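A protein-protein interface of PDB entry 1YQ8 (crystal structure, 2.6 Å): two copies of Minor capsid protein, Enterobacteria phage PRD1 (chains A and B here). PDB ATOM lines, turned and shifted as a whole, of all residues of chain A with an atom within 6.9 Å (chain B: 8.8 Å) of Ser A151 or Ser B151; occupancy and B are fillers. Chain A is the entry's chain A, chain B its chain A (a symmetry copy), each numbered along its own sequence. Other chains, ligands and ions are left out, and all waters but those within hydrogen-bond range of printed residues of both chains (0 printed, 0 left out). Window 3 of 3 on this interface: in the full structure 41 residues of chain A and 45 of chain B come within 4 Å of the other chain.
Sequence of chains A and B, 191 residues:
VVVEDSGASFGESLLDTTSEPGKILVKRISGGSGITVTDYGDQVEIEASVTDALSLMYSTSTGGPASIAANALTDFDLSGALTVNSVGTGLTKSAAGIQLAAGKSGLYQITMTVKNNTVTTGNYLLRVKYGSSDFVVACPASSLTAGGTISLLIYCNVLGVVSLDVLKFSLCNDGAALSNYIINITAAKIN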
ATOM      1  N   GLN A 109      30.608 -11.264 -13.032  1.00  0.00           N
ATOM      2  CA  GLN A 109      31.248 -10.886 -14.290  1.00  0.00           C
ATOM      3  C   GLN A 109      32.573 -11.637 -14.320  1.00  0.00           C
ATOM      4  O   GLN A 109      33.486 -11.323 -13.565  1.00  0.00           O
ATOM      5  CB  GLN A 109      31.477  -9.371 -14.330  1.00  0.00           C
ATOM      6  CG  GLN A 109      32.267  -8.862 -15.520  1.00  0.00           C
ATOM      7  CD  GLN A 109      31.730  -9.355 -16.850  1.00  0.00           C
ATOM      8  OE1 GLN A 109      30.524  -9.348 -17.077  1.00  0.00           O
ATOM      9  NE2 GLN A 109      32.635  -9.769 -17.748  1.00  0.00           N
ATOM     10  N   ILE A 110      32.666 -12.632 -15.197  1.00  0.00           N
ATOM     11  CA  ILE A 110      33.847 -13.484 -15.299  1.00  0.00           C
ATOM     12  C   ILE A 110      34.618 -13.379 -16.610  1.00  0.00           C
ATOM     13  O   ILE A 110      34.030 -13.289 -17.676  1.00  0.00           O
ATOM     14  CB  ILE A 110      33.424 -14.960 -15.087  1.00  0.00           C
ATOM     15  CG1 ILE A 110      32.829 -15.126 -13.692  1.00  0.00           C
ATOM     16  CG2 ILE A 110      34.598 -15.884 -15.272  1.00  0.00           C
ATOM     17  CD1 ILE A 110      31.920 -16.308 -13.559  1.00  0.00           C
ATOM     18  N   THR A 111      35.942 -13.401 -16.524  1.00  0.00           N
ATOM     19  CA  THR A 111      36.788 -13.339 -17.710  1.00  0.00           C
ATOM     20  C   THR A 111      38.013 -14.214 -17.525  1.00  0.00           C
ATOM     21  O   THR A 111      38.699 -14.104 -16.523  1.00  0.00           O
ATOM     22  CB  THR A 111      37.301 -11.886 -18.005  1.00  0.00           C
ATOM     23  OG1 THR A 111      36.217 -11.066 -18.451  1.00  0.00           O
ATOM     24  CG2 THR A 111      38.383 -11.900 -19.088  1.00  0.00           C
ATOM     25  N   MET A 112      38.264 -15.100 -18.480  1.00  0.00           N
ATOM     26  CA  MET A 112      39.455 -15.945 -18.460  1.00  0.00           C
ATOM     27  C   MET A 112      40.141 -15.735 -19.803  1.00  0.00           C
ATOM     28  O   MET A 112      39.527 -15.910 -20.865  1.00  0.00           O
ATOM     29  CB  MET A 112      39.128 -17.435 -18.294  1.00  0.00           C
ATOM     30  CG  MET A 112      40.391 -18.315 -18.364  1.00  0.00           C
ATOM     31  SD  MET A 112      40.205 -20.113 -18.140  1.00  0.00           S
ATOM     32  CE  MET A 112      39.259 -20.562 -19.589  1.00  0.00           C
ATOM     33  N   LEU A 126      38.225 -22.749 -24.761  1.00  0.00           N
ATOM     34  CA  LEU A 126      38.090 -22.203 -23.410  1.00  0.00           C
ATOM     35  C   LEU A 126      36.792 -22.650 -22.728  1.00  0.00           C
ATOM     36  O   LEU A 126      35.761 -22.848 -23.377  1.00  0.00           O
ATOM     37  CB  LEU A 126      38.164 -20.677 -23.456  1.00  0.00           C
ATOM     38  CG  LEU A 126      39.485 -20.087 -23.963  1.00  0.00           C
ATOM     39  CD1 LEU A 126      39.640 -20.301 -25.451  1.00  0.00           C
ATOM     40  CD2 LEU A 126      39.499 -18.611 -23.656  1.00  0.00           C
ATOM     41  N   VAL A 128      34.443 -22.285 -18.882  1.00  0.00           N
ATOM     42  CA  VAL A 128      34.113 -21.882 -17.520  1.00  0.00           C
ATOM     43  C   VAL A 128      32.868 -22.683 -17.167  1.00  0.00           C
ATOM     44  O   VAL A 128      31.970 -22.816 -17.990  1.00  0.00           O
ATOM     45  CB  VAL A 128      33.772 -20.365 -17.464  1.00  0.00           C
ATOM     46  CG1 VAL A 128      33.301 -19.974 -16.079  1.00  0.00           C
ATOM     47  CG2 VAL A 128      34.990 -19.555 -17.868  1.00  0.00           C
ATOM     48  N   VAL A 137      33.747 -21.551 -25.760  1.00  0.00           N
ATOM     49  CA  VAL A 137      34.106 -20.714 -26.902  1.00  0.00           C
ATOM     50  C   VAL A 137      35.458 -21.144 -27.476  1.00  0.00           C
ATOM     51  O   VAL A 137      36.414 -21.383 -26.740  1.00  0.00           O
ATOM     52  CB  VAL A 137      34.157 -19.188 -26.522  1.00  0.00           C
ATOM     53  CG1 VAL A 137      35.387 -18.892 -25.670  1.00  0.00           C
ATOM     54  CG2 VAL A 137      34.132 -18.317 -27.788  1.00  0.00           C
ATOM     55  N   THR A 149      40.031 -15.857 -25.352  1.00  0.00           N
ATOM     56  CA  THR A 149      39.360 -15.117 -24.292  1.00  0.00           C
ATOM     57  C   THR A 149      37.922 -15.596 -24.138  1.00  0.00           C
ATOM     58  O   THR A 149      37.265 -15.970 -25.122  1.00  0.00           O
ATOM     59  CB  THR A 149      39.291 -13.592 -24.634  1.00  0.00           C
ATOM     60  OG1 THR A 149      40.609 -13.061 -24.806  1.00  0.00           O
ATOM     61  CG2 THR A 149      38.569 -12.826 -23.544  1.00  0.00           C
ATOM     62  N   ILE A 150      37.434 -15.605 -22.905  1.00  0.00           N
ATOM     63  CA  ILE A 150      36.042 -15.950 -22.673  1.00  0.00           C
ATOM     64  C   ILE A 150      35.574 -15.068 -21.525  1.00  0.00           C
ATOM     65  O   ILE A 150      36.072 -15.162 -20.401  1.00  0.00           O
ATOM     66  CB  ILE A 150      35.820 -17.455 -22.350  1.00  0.00           C
ATOM     67  CG1 ILE A 150      34.317 -17.755 -22.420  1.00  0.00           C
ATOM     68  CG2 ILE A 150      36.402 -17.818 -20.988  1.00  0.00           C
ATOM     69  CD1 ILE A 150      33.953 -19.195 -22.224  1.00  0.00           C
ATOM     70  N   SER A 151      34.648 -14.167 -21.832  1.00  0.00           N
ATOM     71  CA  SER A 151      34.118 -13.258 -20.834  1.00  0.00           C
ATOM     72  C   SER A 151      32.665 -13.654 -20.608  1.00  0.00           C
ATOM     73  O   SER A 151      31.972 -14.033 -21.543  1.00  0.00           O
ATOM     74  CB  SER A 151      34.242 -11.816 -21.337  1.00  0.00           C
ATOM     75  OG  SER A 151      33.967 -10.872 -20.308  1.00  0.00           O
ATOM     76  N   LEU A 152      32.206 -13.576 -19.368  1.00  0.00           N
ATOM     77  CA  LEU A 152      30.844 -13.974 -19.045  1.00  0.00           C
ATOM     78  C   LEU A 152      30.208 -13.156 -17.936  1.00  0.00           C
ATOM     79  O   LEU A 152      30.872 -12.720 -17.002  1.00  0.00           O
ATOM     80  CB  LEU A 152      30.811 -15.431 -18.575  1.00  0.00           C
ATOM     81  CG  LEU A 152      31.145 -16.647 -19.423  1.00  0.00           C
ATOM     82  CD1 LEU A 152      31.345 -17.826 -18.493  1.00  0.00           C
ATOM     83  CD2 LEU A 152      30.030 -16.932 -20.403  1.00  0.00           C
ATOM     84  N   LEU A 153      28.903 -12.976 -18.048  1.00  0.00           N
ATOM     85  CA  LEU A 153      28.117 -12.288 -17.038  1.00  0.00           C
ATOM     86  C   LEU A 153      27.045 -13.323 -16.766  1.00  0.00           C
ATOM     87  O   LEU A 153      26.151 -13.546 -17.583  1.00  0.00           O
ATOM     88  CB  LEU A 153      27.490 -11.006 -17.578  1.00  0.00           C
ATOM     89  CG  LEU A 153      26.611 -10.335 -16.530  1.00  0.00           C
ATOM     90  CD1 LEU A 153      27.415 -10.088 -15.261  1.00  0.00           C
ATOM     91  CD2 LEU A 153      26.077  -9.045 -17.074  1.00  0.00           C
ATOM     92  N   TYR B 108      25.227  -0.959 -20.443  1.00  0.00           N
ATOM     93  CA  TYR B 108      24.732  -2.294 -20.179  1.00  0.00           C
ATOM     94  C   TYR B 108      25.754  -3.397 -20.415  1.00  0.00           C
ATOM     95  O   TYR B 108      26.436  -3.413 -21.430  1.00  0.00           O
ATOM     96  CB  TYR B 108      23.494  -2.564 -21.044  1.00  0.00           C
ATOM     97  CG  TYR B 108      22.278  -1.767 -20.641  1.00  0.00           C
ATOM     98  CD1 TYR B 108      22.206  -0.397 -20.883  1.00  0.00           C
ATOM     99  CD2 TYR B 108      21.218  -2.377 -19.969  1.00  0.00           C
ATOM    100  CE1 TYR B 108      21.107   0.346 -20.455  1.00  0.00           C
ATOM    101  CE2 TYR B 108      20.119  -1.645 -19.540  1.00  0.00           C
ATOM    102  CZ  TYR B 108      20.068  -0.287 -19.780  1.00  0.00           C
ATOM    103  OH  TYR B 108      19.001   0.443 -19.313  1.00  0.00           O
ATOM    104  N   GLN B 109      25.841  -4.324 -19.467  1.00  0.00           N
ATOM    105  CA  GLN B 109      26.750  -5.465 -19.567  1.00  0.00           C
ATOM    106  C   GLN B 109      25.885  -6.641 -20.004  1.00  0.00           C
ATOM    107  O   GLN B 109      25.073  -7.139 -19.232  1.00  0.00           O
ATOM    108  CB  GLN B 109      27.402  -5.739 -18.208  1.00  0.00           C
ATOM    109  CG  GLN B 109      28.258  -6.989 -18.136  1.00  0.00           C
ATOM    110  CD  GLN B 109      29.286  -7.075 -19.247  1.00  0.00           C
ATOM    111  OE1 GLN B 109      29.953  -6.094 -19.558  1.00  0.00           O
ATOM    112  NE2 GLN B 109      29.432  -8.268 -19.842  1.00  0.00           N
ATOM    113  N   ILE B 110      26.068  -7.077 -21.246  1.00  0.00           N
ATOM    114  CA  ILE B 110      25.272  -8.153 -21.828  1.00  0.00           C
ATOM    115  C   ILE B 110      26.040  -9.425 -22.169  1.00  0.00           C
ATOM    116  O   ILE B 110      27.155  -9.371 -22.660  1.00  0.00           O
ATOM    117  CB  ILE B 110      24.580  -7.631 -23.113  1.00  0.00           C
ATOM    118  CG1 ILE B 110      23.646  -6.478 -22.758  1.00  0.00           C
ATOM    119  CG2 ILE B 110      23.818  -8.735 -23.796  1.00  0.00           C
ATOM    120  CD1 ILE B 110      23.352  -5.564 -23.907  1.00  0.00           C
ATOM    121  N   THR B 111      25.429 -10.575 -21.911  1.00  0.00           N
ATOM    122  CA  THR B 111      26.050 -11.858 -22.220  1.00  0.00           C
ATOM    123  C   THR B 111      24.999 -12.847 -22.690  1.00  0.00           C
ATOM    124  O   THR B 111      23.987 -13.025 -22.032  1.00  0.00           O
ATOM    125  CB  THR B 111      26.758 -12.498 -20.976  1.00  0.00           C
ATOM    126  OG1 THR B 111      27.931 -11.748 -20.643  1.00  0.00           O
ATOM    127  CG2 THR B 111      27.167 -13.945 -21.265  1.00  0.00           C
ATOM    128  N   MET B 112      25.229 -13.462 -23.842  1.00  0.00           N
ATOM    129  CA  MET B 112      24.336 -14.494 -24.362  1.00  0.00           C
ATOM    130  C   MET B 112      25.213 -15.707 -24.640  1.00  0.00           C
ATOM    131  O   MET B 112      26.212 -15.618 -25.368  1.00  0.00           O
ATOM    132  CB  MET B 112      23.636 -14.078 -25.663  1.00  0.00           C
ATOM    133  CG  MET B 112      22.768 -15.212 -26.241  1.00  0.00           C
ATOM    134  SD  MET B 112      21.820 -14.885 -27.762  1.00  0.00           S
ATOM    135  CE  MET B 112      23.127 -14.659 -28.960  1.00  0.00           C
ATOM    136  N   THR B 113      24.855 -16.838 -24.047  1.00  0.00           N
ATOM    137  CA  THR B 113      25.625 -18.062 -24.237  1.00  0.00           C
ATOM    138  C   THR B 113      24.766 -19.162 -24.833  1.00  0.00           C
ATOM    139  O   THR B 113      23.541 -19.105 -24.782  1.00  0.00           O
ATOM    140  CB  THR B 113      26.210 -18.581 -22.890  1.00  0.00           C
ATOM    141  OG1 THR B 113      25.189 -18.580 -21.887  1.00  0.00           O
ATOM    142  CG2 THR B 113      27.370 -17.722 -22.428  1.00  0.00           C
ATOM    143  N   LEU B 126      26.573 -15.932 -33.332  1.00  0.00           N
ATOM    144  CA  LEU B 126      25.824 -15.236 -32.285  1.00  0.00           C
ATOM    145  C   LEU B 126      25.601 -13.756 -32.617  1.00  0.00           C
ATOM    146  O   LEU B 126      26.432 -13.109 -33.261  1.00  0.00           O
ATOM    147  CB  LEU B 126      26.549 -15.374 -30.946  1.00  0.00           C
ATOM    148  CG  LEU B 126      26.694 -16.802 -30.409  1.00  0.00           C
ATOM    149  CD1 LEU B 126      27.698 -17.589 -31.218  1.00  0.00           C
ATOM    150  CD2 LEU B 126      27.142 -16.729 -28.972  1.00  0.00           C
ATOM    151  N   VAL B 128      23.699  -9.968 -31.041  1.00  0.00           N
ATOM    152  CA  VAL B 128      22.953  -9.086 -30.152  1.00  0.00           C
ATOM    153  C   VAL B 128      22.800  -7.787 -30.929  1.00  0.00           C
ATOM    154  O   VAL B 128      23.745  -7.338 -31.567  1.00  0.00           O
ATOM    155  CB  VAL B 128      23.760  -8.807 -28.852  1.00  0.00           C
ATOM    156  CG1 VAL B 128      23.047  -7.789 -27.988  1.00  0.00           C
ATOM    157  CG2 VAL B 128      23.969 -10.104 -28.094  1.00  0.00           C
ATOM    158  N   PHE B 135      25.991  -6.296 -32.888  1.00  0.00           N
ATOM    159  CA  PHE B 135      27.263  -6.932 -32.573  1.00  0.00           C
ATOM    160  C   PHE B 135      27.263  -8.440 -32.830  1.00  0.00           C
ATOM    161  O   PHE B 135      26.308  -9.142 -32.479  1.00  0.00           O
ATOM    162  CB  PHE B 135      27.616  -6.607 -31.121  1.00  0.00           C
ATOM    163  CG  PHE B 135      27.347  -5.173 -30.751  1.00  0.00           C
ATOM    164  CD1 PHE B 135      26.103  -4.789 -30.250  1.00  0.00           C
ATOM    165  CD2 PHE B 135      28.316  -4.190 -30.952  1.00  0.00           C
ATOM    166  CE1 PHE B 135      25.821  -3.448 -29.959  1.00  0.00           C
ATOM    167  CE2 PHE B 135      28.046  -2.853 -30.666  1.00  0.00           C
ATOM    168  CZ  PHE B 135      26.796  -2.483 -30.168  1.00  0.00           C
ATOM    169  N   VAL B 136      28.340  -8.932 -33.440  1.00  0.00           N
ATOM    170  CA  VAL B 136      28.445 -10.349 -33.775  1.00  0.00           C
ATOM    171  C   VAL B 136      29.740 -11.073 -33.363  1.00  0.00           C
ATOM    172  O   VAL B 136      30.708 -10.458 -32.920  1.00  0.00           O
ATOM    173  CB  VAL B 136      28.262 -10.533 -35.286  1.00  0.00           C
ATOM    174  CG1 VAL B 136      26.962  -9.884 -35.729  1.00  0.00           C
ATOM    175  CG2 VAL B 136      29.447  -9.926 -36.026  1.00  0.00           C
ATOM    176  N   VAL B 137      29.725 -12.394 -33.520  1.00  0.00           N
ATOM    177  CA  VAL B 137      30.870 -13.247 -33.216  1.00  0.00           C
ATOM    178  C   VAL B 137      30.574 -14.698 -33.601  1.00  0.00           C
ATOM    179  O   VAL B 137      29.499 -15.224 -33.318  1.00  0.00           O
ATOM    180  CB  VAL B 137      31.270 -13.177 -31.696  1.00  0.00           C
ATOM    181  CG1 VAL B 137      30.246 -13.916 -30.840  1.00  0.00           C
ATOM    182  CG2 VAL B 137      32.684 -13.741 -31.485  1.00  0.00           C
ATOM    183  N   CYS B 139      31.649 -18.696 -33.322  1.00  0.00           N
ATOM    184  CA  CYS B 139      32.377 -19.584 -32.439  1.00  0.00           C
ATOM    185  C   CYS B 139      32.533 -20.987 -33.007  1.00  0.00           C
ATOM    186  O   CYS B 139      31.573 -21.756 -33.073  1.00  0.00           O
ATOM    187  CB  CYS B 139      31.675 -19.642 -31.081  1.00  0.00           C
ATOM    188  SG  CYS B 139      31.506 -18.017 -30.299  1.00  0.00           S
ATOM    189  N   GLY B 148      28.698 -21.507 -27.908  1.00  0.00           N
ATOM    190  CA  GLY B 148      29.246 -20.203 -28.217  1.00  0.00           C
ATOM    191  C   GLY B 148      28.893 -19.192 -27.150  1.00  0.00           C
ATOM    192  O   GLY B 148      28.025 -19.430 -26.318  1.00  0.00           O
ATOM    193  N   THR B 149      29.556 -18.045 -27.188  1.00  0.00           N
ATOM    194  CA  THR B 149      29.343 -17.002 -26.195  1.00  0.00           C
ATOM    195  C   THR B 149      29.575 -15.628 -26.809  1.00  0.00           C
ATOM    196  O   THR B 149      30.436 -15.458 -27.687  1.00  0.00           O
ATOM    197  CB  THR B 149      30.358 -17.143 -25.011  1.00  0.00           C
ATOM    198  OG1 THR B 149      30.212 -18.418 -24.380  1.00  0.00           O
ATOM    199  CG2 THR B 149      30.152 -16.040 -23.992  1.00  0.00           C
ATOM    200  N   ILE B 150      28.799 -14.647 -26.367  1.00  0.00           N
ATOM    201  CA  ILE B 150      29.015 -13.284 -26.822  1.00  0.00           C
ATOM    202  C   ILE B 150      28.718 -12.389 -25.628  1.00  0.00           C
ATOM    203  O   ILE B 150      27.591 -12.338 -25.131  1.00  0.00           O
ATOM    204  CB  ILE B 150      28.143 -12.893 -28.048  1.00  0.00           C
ATOM    205  CG1 ILE B 150      28.661 -11.564 -28.614  1.00  0.00           C
ATOM    206  CG2 ILE B 150      26.667 -12.803 -27.668  1.00  0.00           C
ATOM    207  CD1 ILE B 150      27.975 -11.103 -29.864  1.00  0.00           C
ATOM    208  N   SER B 151      29.756 -11.723 -25.135  1.00  0.00           N
ATOM    209  CA  SER B 151      29.613 -10.839 -23.994  1.00  0.00           C
ATOM    210  C   SER B 151      29.835  -9.423 -24.507  1.00  0.00           C
ATOM    211  O   SER B 151      30.670  -9.199 -25.374  1.00  0.00           O
ATOM    212  CB  SER B 151      30.639 -11.221 -22.920  1.00  0.00           C
ATOM    213  OG  SER B 151      30.386 -10.553 -21.690  1.00  0.00           O
ATOM    214  N   LEU B 152      29.082  -8.468 -23.981  1.00  0.00           N
ATOM    215  CA  LEU B 152      29.190  -7.090 -24.437  1.00  0.00           C
ATOM    216  C   LEU B 152      28.961  -6.059 -23.347  1.00  0.00           C
ATOM    217  O   LEU B 152      28.165  -6.259 -22.435  1.00  0.00           O
ATOM    218  CB  LEU B 152      28.149  -6.805 -25.522  1.00  0.00           C
ATOM    219  CG  LEU B 152      28.107  -7.436 -26.904  1.00  0.00           C
ATOM    220  CD1 LEU B 152      26.740  -7.167 -27.501  1.00  0.00           C
ATOM    221  CD2 LEU B 152      29.190  -6.857 -27.784  1.00  0.00           C
ATOM    222  N   LEU B 153      29.659  -4.944 -23.472  1.00  0.00           N
ATOM    223  CA  LEU B 153      29.506  -3.817 -22.568  1.00  0.00           C
ATOM    224  C   LEU B 153      29.237  -2.700 -23.555  1.00  0.00           C
ATOM    225  O   LEU B 153      30.133  -2.250 -24.270  1.00  0.00           O
ATOM    226  CB  LEU B 153      30.786  -3.535 -21.787  1.00  0.00           C
ATOM    227  CG  LEU B 153      30.633  -2.308 -20.897  1.00  0.00           C
ATOM    228  CD1 LEU B 153      29.430  -2.480 -19.980  1.00  0.00           C
ATOM    229  CD2 LEU B 153      31.883  -2.112 -20.094  1.00  0.00           C
ATOM    230  N   ILE B 154      27.993  -2.272 -23.627  1.00  0.00           N
ATOM    231  CA  ILE B 154      27.651  -1.241 -24.580  1.00  0.00           C
ATOM    232  C   ILE B 154      26.880  -0.079 -23.970  1.00  0.00           C
ATOM    233  O   ILE B 154      26.388  -0.154 -22.852  1.00  0.00           O
ATOM    234  CB  ILE B 154      26.825  -1.850 -25.745  1.00  0.00           C
ATOM    235  CG1 ILE B 154      25.561  -2.513 -25.202  1.00  0.00           C
ATOM    236  CG2 ILE B 154      27.648  -2.877 -26.490  1.00  0.00           C
ATOM    237  CD1 ILE B 154      24.706  -3.167 -26.263  1.00  0.00           C
ATOM    238  N   PHE B 169      17.896 -10.541 -29.681  1.00  0.00           N
ATOM    239  CA  PHE B 169      18.922 -11.591 -29.612  1.00  0.00           C
ATOM    240  C   PHE B 169      18.781 -12.675 -30.677  1.00  0.00           C
ATOM    241  O   PHE B 169      17.686 -12.924 -31.177  1.00  0.00           O
ATOM    242  CB  PHE B 169      18.928 -12.239 -28.222  1.00  0.00           C
ATOM    243  CG  PHE B 169      19.397 -11.324 -27.133  1.00  0.00           C
ATOM    244  CD1 PHE B 169      18.516 -10.443 -26.520  1.00  0.00           C
ATOM    245  CD2 PHE B 169      20.737 -11.309 -26.752  1.00  0.00           C
ATOM    246  CE1 PHE B 169      18.958  -9.561 -25.553  1.00  0.00           C
ATOM    247  CE2 PHE B 169      21.188 -10.426 -25.784  1.00  0.00           C
ATOM    248  CZ  PHE B 169      20.298  -9.552 -25.185  1.00  0.00           C
ATOM    249  N   THR B 186      21.755 -12.683 -20.289  1.00  0.00           N
ATOM    250  CA  THR B 186      21.732 -11.859 -19.096  1.00  0.00           C
ATOM    251  C   THR B 186      22.084 -10.441 -19.490  1.00  0.00           C
ATOM    252  O   THR B 186      23.042 -10.210 -20.224  1.00  0.00           O
ATOM    253  CB  THR B 186      22.759 -12.312 -18.031  1.00  0.00           C
ATOM    254  OG1 THR B 186      22.623 -13.716 -17.768  1.00  0.00           O
ATOM    255  CG2 THR B 186      22.532 -11.545 -16.741  1.00  0.00           C
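The side-chain amide nitrogen (NE2) of Gln B109 lies within hydrogen-bond range of the side-chain amide oxygen (OE1) of Gln A109, at 3.2 Å.
OG1 of Thr B111 sits at hydrogen-bond distance from N of Leu A153, at 3.0 Å.
The side-chain amide nitrogen (NE2) of Gln A109 lies within hydrogen-bond range of the side-chain hydroxyl (OG) of Ser A151 (3.1 Å).
The side-chain hydroxyl (OG) of Ser A151 is in hydrogen-bond range of the side-chain hydroxyl (OG1) of Thr A111 (2.9 Å).
N of Leu A126 lies within hydrogen-bond range of O of Val A137 (3.0 Å).
OG of Ser B151 is in hydrogen-bond range of OG1 of Thr B111 (2.9 Å).
O of Thr B111 is in hydrogen-bond range of N of Thr B186 (2.9 Å).
The side-chain sulfur (SG) of Cys B139 is in hydrogen-bond range of the backbone NH (N) of Thr B149, 3.7 Å away.
Among the printed residues, merely in contact across the chains: Val A137 with Cys B139, Ser A151 with Thr B149, Ser A151 with Ser B151, Leu A152 with Thr B111, Leu A152 with Thr B113, Leu A152 with Thr B149, Leu A153 with Gln B109 and Leu A153 with Thr B186.
Of the printed residues of chain B, Gln A109 touches Gln B109 (3.2 Å).
Ser A151 touches just these residues of chain B: Thr B149 (3.7 Å) and Ser B151 (3.4 Å).
Printed residues of chain B within 4 Å of Leu A153: Gln B109, Thr B111 and Thr B186.
Of the printed residues of chain A, Gln B109 touches Gln A109 (3.2 Å) and Leu A153 (3.0 Å).
Ile B110 touches none of the printed residues of chain A.
Of the printed residues of chain A, Thr B149 touches Ser A151 (3.7 Å) and Leu A152 (3.7 Å).
Ile B150 touches none of the printed residues of chain A.
Of the printed residues of chain A, Ser B151 touches Ser A151 (3.4 Å).
Of the printed residues of chain A, Thr B186 touches Leu A153 (3.5 Å).
The nearest printed residue of chain A that does not touch Thr B149 is Ile A150 (4.4 Å).
Hydrophobic or aromatic side chains of chain A within 4 Å of the printed part of chain B: Val A137, Leu A152 and Leu A153.
Of the 21 printed residues of chain B, 7 touch a printed residue of chain A.
Printed residues of chain B that touch a printed residue of chain A: Gln B109, Thr B111, Thr B113, Cys B139, Thr B149, Ser B151 and Thr B186.
Among the printed residues, 10 pairs touch across the chains.
Among the printed residues, no Asp or Glu carboxylate lies within 4 Å of a Lys or Arg side-chain nitrogen of the other chain.
Gln B109 touches its own counterpart, Gln A109.
Ser A151 touches Thr B149, but with the chains exchanged Thr A149 does not touch Ser B151 (8.1 Å).
Leu A152 touches Thr B149, but with the chains exchanged Thr A149 does not touch Leu B152 (10.4 Å).
Leu A153 touches Gln B109, but with the chains exchanged Gln A109 does not touch Leu B153 (7.5 Å).
12 positions are printed for both chains.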
